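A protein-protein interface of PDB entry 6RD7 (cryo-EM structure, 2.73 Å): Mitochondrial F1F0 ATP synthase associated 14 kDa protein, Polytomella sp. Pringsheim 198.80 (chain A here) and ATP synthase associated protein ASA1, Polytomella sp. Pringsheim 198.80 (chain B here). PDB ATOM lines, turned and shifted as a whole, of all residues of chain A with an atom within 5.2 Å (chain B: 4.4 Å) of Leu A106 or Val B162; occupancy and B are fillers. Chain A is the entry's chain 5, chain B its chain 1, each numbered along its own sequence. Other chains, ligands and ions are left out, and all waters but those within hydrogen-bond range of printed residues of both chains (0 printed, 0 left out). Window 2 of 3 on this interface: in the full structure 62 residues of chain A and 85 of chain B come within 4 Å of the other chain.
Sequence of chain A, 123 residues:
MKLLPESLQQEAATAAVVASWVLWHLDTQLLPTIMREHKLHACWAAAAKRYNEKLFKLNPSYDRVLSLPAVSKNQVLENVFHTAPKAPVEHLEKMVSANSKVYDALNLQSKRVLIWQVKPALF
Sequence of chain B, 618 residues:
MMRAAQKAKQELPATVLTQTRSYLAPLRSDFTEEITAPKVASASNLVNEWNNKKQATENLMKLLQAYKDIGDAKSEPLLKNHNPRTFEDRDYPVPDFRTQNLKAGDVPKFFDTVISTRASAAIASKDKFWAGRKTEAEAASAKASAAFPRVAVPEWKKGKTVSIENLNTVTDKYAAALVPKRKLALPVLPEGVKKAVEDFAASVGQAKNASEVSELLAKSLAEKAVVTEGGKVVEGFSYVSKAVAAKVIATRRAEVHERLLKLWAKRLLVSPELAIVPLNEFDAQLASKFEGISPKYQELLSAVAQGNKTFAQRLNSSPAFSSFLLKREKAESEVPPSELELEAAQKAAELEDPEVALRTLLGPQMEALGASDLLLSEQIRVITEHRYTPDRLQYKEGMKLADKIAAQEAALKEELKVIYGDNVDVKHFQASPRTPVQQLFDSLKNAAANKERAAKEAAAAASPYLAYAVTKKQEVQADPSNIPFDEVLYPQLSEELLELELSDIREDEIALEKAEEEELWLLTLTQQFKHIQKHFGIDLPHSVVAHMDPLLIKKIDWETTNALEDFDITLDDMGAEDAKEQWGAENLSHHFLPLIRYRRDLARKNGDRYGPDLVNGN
N of Ile B164 lies close to ND2 of Asn A107 (3.4 Å).
O of Val B162 sits close to ND2 of Asn A107 (2.4 Å).
N of Val B162 is in hydrogen-bond range of O of Leu A106, at 2.6 Å.
Pro B154 touches Val A102.
Ile B164 touches Tyr A103 (CD1 to CE1, 3.7 Å).
CD1 of Leu B167 touches CD1 of Tyr A103 (3.6 Å).
Leu A106 touches Trp B156 (CD1 to CE2, 3.5 Å).
Leu A106 touches Thr B161 (O to CB, 3.3 Å).
ND2 of Asn A107 touches C of Ser B163 (3.6 Å).
CD1 of Leu A108 touches OG1 of Thr B161, at 3.8 Å.
Lys A101 touches none of the printed residues of chain B.
Printed residues of chain B within 4 Å of Val A102: Pro B154 (3.9 Å).
Of the printed residues of chain A, Pro B154 touches Val A102 (3.9 Å).
Glu B155 touches none of the printed residues of chain A.
Printed residues of chain A within 4 Å of Trp B156: Leu A106.
Printed residues of chain A within 4 Å of Val B162: Leu A106 (2.6 Å) and Asn A107 (2.4 Å).
Of the printed residues of chain A, Ser B163 touches Asn A107 (3.6 Å).
Of the printed residues of chain A, Ile B164 touches Tyr A103 (3.7 Å) and Asn A107 (3.4 Å).
The nearest printed residue of chain B that does not touch Leu A108 is Val B162 (4.9 Å).
Printed residues of chain B that touch a printed residue of chain A: Pro B154, Trp B156, Thr B161, Val B162, Ser B163, Ile B164 and Leu B167.
Hydrophobic or aromatic side chains of chain B that line the printed part of chain A: Pro B154, Trp B156, Val B162, Ile B164 and Leu B167.
Of the 9 printed residues of chain A, 5 touch a printed residue of chain B.
Hydrophobic or aromatic side chains of chain A that line the printed part of chain B: Val A102, Tyr A103, Leu A106 and Leu A108.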
ATOM      1  N   LYS A 101     -14.188 -19.093  25.804  1.00  0.00           N
ATOM      2  CA  LYS A 101     -15.253 -18.246  25.279  1.00  0.00           C
ATOM      3  C   LYS A 101     -15.444 -18.472  23.787  1.00  0.00           C
ATOM      4  O   LYS A 101     -16.575 -18.438  23.286  1.00  0.00           O
ATOM      5  CB  LYS A 101     -14.938 -16.779  25.555  1.00  0.00           C
ATOM      6  CG  LYS A 101     -14.853 -16.422  27.019  1.00  0.00           C
ATOM      7  CD  LYS A 101     -14.734 -14.924  27.204  1.00  0.00           C
ATOM      8  CE  LYS A 101     -13.521 -14.374  26.482  1.00  0.00           C
ATOM      9  NZ  LYS A 101     -13.346 -12.924  26.740  1.00  0.00           N
ATOM     10  N   VAL A 102     -14.343 -18.708  23.067  1.00  0.00           N
ATOM     11  CA  VAL A 102     -14.426 -19.031  21.639  1.00  0.00           C
ATOM     12  C   VAL A 102     -15.182 -20.342  21.421  1.00  0.00           C
ATOM     13  O   VAL A 102     -16.021 -20.449  20.517  1.00  0.00           O
ATOM     14  CB  VAL A 102     -13.014 -19.070  21.025  1.00  0.00           C
ATOM     15  CG1 VAL A 102     -13.021 -19.683  19.639  1.00  0.00           C
ATOM     16  CG2 VAL A 102     -12.435 -17.678  20.971  1.00  0.00           C
ATOM     17  N   TYR A 103     -14.927 -21.343  22.268  1.00  0.00           N
ATOM     18  CA  TYR A 103     -15.647 -22.611  22.189  1.00  0.00           C
ATOM     19  C   TYR A 103     -17.118 -22.429  22.531  1.00  0.00           C
ATOM     20  O   TYR A 103     -17.990 -23.015  21.883  1.00  0.00           O
ATOM     21  CB  TYR A 103     -15.015 -23.644  23.127  1.00  0.00           C
ATOM     22  CG  TYR A 103     -15.828 -24.921  23.249  1.00  0.00           C
ATOM     23  CD1 TYR A 103     -15.744 -25.904  22.279  1.00  0.00           C
ATOM     24  CD2 TYR A 103     -16.678 -25.143  24.333  1.00  0.00           C
ATOM     25  CE1 TYR A 103     -16.481 -27.056  22.372  1.00  0.00           C
ATOM     26  CE2 TYR A 103     -17.429 -26.288  24.423  1.00  0.00           C
ATOM     27  CZ  TYR A 103     -17.321 -27.242  23.441  1.00  0.00           C
ATOM     28  OH  TYR A 103     -18.057 -28.393  23.520  1.00  0.00           O
ATOM     29  N   ASP A 104     -17.406 -21.653  23.581  1.00  0.00           N
ATOM     30  CA  ASP A 104     -18.779 -21.430  24.021  1.00  0.00           C
ATOM     31  C   ASP A 104     -19.593 -20.717  22.948  1.00  0.00           C
ATOM     32  O   ASP A 104     -20.785 -20.982  22.773  1.00  0.00           O
ATOM     33  CB  ASP A 104     -18.785 -20.618  25.315  1.00  0.00           C
ATOM     34  CG  ASP A 104     -18.508 -21.459  26.537  1.00  0.00           C
ATOM     35  OD1 ASP A 104     -18.427 -20.887  27.643  1.00  0.00           O
ATOM     36  OD2 ASP A 104     -18.372 -22.692  26.397  1.00  0.00           O
ATOM     37  N   ALA A 105     -18.951 -19.818  22.204  1.00  0.00           N
ATOM     38  CA  ALA A 105     -19.677 -19.088  21.179  1.00  0.00           C
ATOM     39  C   ALA A 105     -19.815 -19.896  19.895  1.00  0.00           C
ATOM     40  O   ALA A 105     -20.910 -19.984  19.331  1.00  0.00           O
ATOM     41  CB  ALA A 105     -18.987 -17.755  20.904  1.00  0.00           C
ATOM     42  N   LEU A 106     -18.730 -20.503  19.413  1.00  0.00           N
ATOM     43  CA  LEU A 106     -18.656 -20.912  18.015  1.00  0.00           C
ATOM     44  C   LEU A 106     -18.505 -22.415  17.807  1.00  0.00           C
ATOM     45  O   LEU A 106     -17.972 -22.830  16.778  1.00  0.00           O
ATOM     46  CB  LEU A 106     -17.501 -20.191  17.328  1.00  0.00           C
ATOM     47  CG  LEU A 106     -17.371 -18.709  17.643  1.00  0.00           C
ATOM     48  CD1 LEU A 106     -15.966 -18.248  17.372  1.00  0.00           C
ATOM     49  CD2 LEU A 106     -18.374 -17.930  16.828  1.00  0.00           C
ATOM     50  N   ASN A 107     -18.943 -23.243  18.744  1.00  0.00           N
ATOM     51  CA  ASN A 107     -18.926 -24.685  18.540  1.00  0.00           C
ATOM     52  C   ASN A 107     -20.349 -25.216  18.543  1.00  0.00           C
ATOM     53  O   ASN A 107     -21.161 -24.810  19.379  1.00  0.00           O
ATOM     54  CB  ASN A 107     -18.097 -25.397  19.605  1.00  0.00           C
ATOM     55  CG  ASN A 107     -17.802 -26.837  19.245  1.00  0.00           C
ATOM     56  OD1 ASN A 107     -18.436 -27.757  19.754  1.00  0.00           O
ATOM     57  ND2 ASN A 107     -16.826 -27.043  18.374  1.00  0.00           N
ATOM     58  N   LEU A 108     -20.637 -26.140  17.622  1.00  0.00           N
ATOM     59  CA  LEU A 108     -22.006 -26.605  17.424  1.00  0.00           C
ATOM     60  C   LEU A 108     -22.495 -27.443  18.596  1.00  0.00           C
ATOM     61  O   LEU A 108     -23.704 -27.543  18.835  1.00  0.00           O
ATOM     62  CB  LEU A 108     -22.100 -27.401  16.125  1.00  0.00           C
ATOM     63  CG  LEU A 108     -21.942 -26.558  14.862  1.00  0.00           C
ATOM     64  CD1 LEU A 108     -21.632 -27.429  13.657  1.00  0.00           C
ATOM     65  CD2 LEU A 108     -23.194 -25.737  14.632  1.00  0.00           C
ATOM     66  N   VAL A 113     -24.278 -21.905  22.208  1.00  0.00           N
ATOM     67  CA  VAL A 113     -23.778 -21.586  20.877  1.00  0.00           C
ATOM     68  C   VAL A 113     -24.562 -20.410  20.301  1.00  0.00           C
ATOM     69  O   VAL A 113     -25.783 -20.302  20.474  1.00  0.00           O
ATOM     70  CB  VAL A 113     -23.840 -22.841  19.981  1.00  0.00           C
ATOM     71  CG1 VAL A 113     -25.230 -23.451  19.974  1.00  0.00           C
ATOM     72  CG2 VAL A 113     -23.372 -22.561  18.557  1.00  0.00           C
ATOM     73  N   PRO B 154      -7.264 -20.527  17.737  1.00  0.00           N
ATOM     74  CA  PRO B 154      -8.107 -21.472  16.997  1.00  0.00           C
ATOM     75  C   PRO B 154      -8.564 -20.895  15.666  1.00  0.00           C
ATOM     76  O   PRO B 154      -8.891 -19.713  15.557  1.00  0.00           O
ATOM     77  CB  PRO B 154      -9.288 -21.711  17.943  1.00  0.00           C
ATOM     78  CG  PRO B 154      -9.260 -20.587  18.892  1.00  0.00           C
ATOM     79  CD  PRO B 154      -7.830 -20.229  19.060  1.00  0.00           C
ATOM     80  N   GLU B 155      -8.566 -21.749  14.650  1.00  0.00           N
ATOM     81  CA  GLU B 155      -8.947 -21.344  13.307  1.00  0.00           C
ATOM     82  C   GLU B 155     -10.448 -21.113  13.226  1.00  0.00           C
ATOM     83  O   GLU B 155     -11.244 -22.007  13.518  1.00  0.00           O
ATOM     84  CB  GLU B 155      -8.517 -22.422  12.320  1.00  0.00           C
ATOM     85  CG  GLU B 155      -8.821 -22.165  10.870  1.00  0.00           C
ATOM     86  CD  GLU B 155      -8.385 -23.330  10.003  1.00  0.00           C
ATOM     87  OE1 GLU B 155      -7.873 -24.324  10.564  1.00  0.00           O
ATOM     88  OE2 GLU B 155      -8.557 -23.260   8.769  1.00  0.00           O
ATOM     89  N   TRP B 156     -10.831 -19.904  12.831  1.00  0.00           N
ATOM     90  CA  TRP B 156     -12.229 -19.509  12.753  1.00  0.00           C
ATOM     91  C   TRP B 156     -12.475 -18.828  11.417  1.00  0.00           C
ATOM     92  O   TRP B 156     -11.982 -17.721  11.185  1.00  0.00           O
ATOM     93  CB  TRP B 156     -12.592 -18.576  13.910  1.00  0.00           C
ATOM     94  CG  TRP B 156     -14.007 -18.113  13.909  1.00  0.00           C
ATOM     95  CD1 TRP B 156     -15.096 -18.811  13.493  1.00  0.00           C
ATOM     96  CD2 TRP B 156     -14.490 -16.845  14.358  1.00  0.00           C
ATOM     97  NE1 TRP B 156     -16.228 -18.054  13.642  1.00  0.00           N
ATOM     98  CE2 TRP B 156     -15.881 -16.840  14.170  1.00  0.00           C
ATOM     99  CE3 TRP B 156     -13.879 -15.711  14.896  1.00  0.00           C
ATOM    100  CZ2 TRP B 156     -16.673 -15.751  14.507  1.00  0.00           C
ATOM    101  CZ3 TRP B 156     -14.666 -14.631  15.227  1.00  0.00           C
ATOM    102  CH2 TRP B 156     -16.048 -14.659  15.032  1.00  0.00           C
ATOM    103  N   THR B 161     -18.151 -22.582  11.865  1.00  0.00           N
ATOM    104  CA  THR B 161     -17.988 -22.792  13.292  1.00  0.00           C
ATOM    105  C   THR B 161     -16.559 -23.233  13.602  1.00  0.00           C
ATOM    106  O   THR B 161     -15.710 -23.357  12.716  1.00  0.00           O
ATOM    107  CB  THR B 161     -18.993 -23.824  13.794  1.00  0.00           C
ATOM    108  OG1 THR B 161     -18.669 -25.112  13.259  1.00  0.00           O
ATOM    109  CG2 THR B 161     -20.397 -23.442  13.367  1.00  0.00           C
ATOM    110  N   VAL B 162     -16.293 -23.466  14.882  1.00  0.00           N
ATOM    111  CA  VAL B 162     -14.967 -23.845  15.355  1.00  0.00           C
ATOM    112  C   VAL B 162     -15.041 -25.258  15.912  1.00  0.00           C
ATOM    113  O   VAL B 162     -15.810 -25.527  16.841  1.00  0.00           O
ATOM    114  CB  VAL B 162     -14.447 -22.861  16.413  1.00  0.00           C
ATOM    115  CG1 VAL B 162     -13.126 -23.337  16.965  1.00  0.00           C
ATOM    116  CG2 VAL B 162     -14.294 -21.481  15.817  1.00  0.00           C
ATOM    117  N   SER B 163     -14.242 -26.161  15.352  1.00  0.00           N
ATOM    118  CA  SER B 163     -14.271 -27.552  15.779  1.00  0.00           C
ATOM    119  C   SER B 163     -13.505 -27.737  17.082  1.00  0.00           C
ATOM    120  O   SER B 163     -12.584 -26.979  17.393  1.00  0.00           O
ATOM    121  CB  SER B 163     -13.684 -28.448  14.693  1.00  0.00           C
ATOM    122  OG  SER B 163     -12.308 -28.182  14.507  1.00  0.00           O
ATOM    123  N   ILE B 164     -13.895 -28.761  17.842  1.00  0.00           N
ATOM    124  CA  ILE B 164     -13.283 -29.016  19.143  1.00  0.00           C
ATOM    125  C   ILE B 164     -11.880 -29.589  18.966  1.00  0.00           C
ATOM    126  O   ILE B 164     -10.984 -29.352  19.790  1.00  0.00           O
ATOM    127  CB  ILE B 164     -14.204 -29.935  19.975  1.00  0.00           C
ATOM    128  CG1 ILE B 164     -13.596 -30.316  21.325  1.00  0.00           C
ATOM    129  CG2 ILE B 164     -14.597 -31.176  19.188  1.00  0.00           C
ATOM    130  CD1 ILE B 164     -13.371 -29.146  22.230  1.00  0.00           C
ATOM    131  N   LEU B 167      -9.374 -26.727  18.602  1.00  0.00           N
ATOM    132  CA  LEU B 167      -9.133 -26.127  19.910  1.00  0.00           C
ATOM    133  C   LEU B 167      -8.234 -27.011  20.763  1.00  0.00           C
ATOM    134  O   LEU B 167      -7.390 -26.512  21.519  1.00  0.00           O
ATOM    135  CB  LEU B 167     -10.461 -25.881  20.618  1.00  0.00           C
ATOM    136  CG  LEU B 167     -11.321 -24.724  20.120  1.00  0.00           C
ATOM    137  CD1 LEU B 167     -12.782 -25.017  20.362  1.00  0.00           C
ATOM    138  CD2 LEU B 167     -10.921 -23.446  20.817  1.00  0.00           C
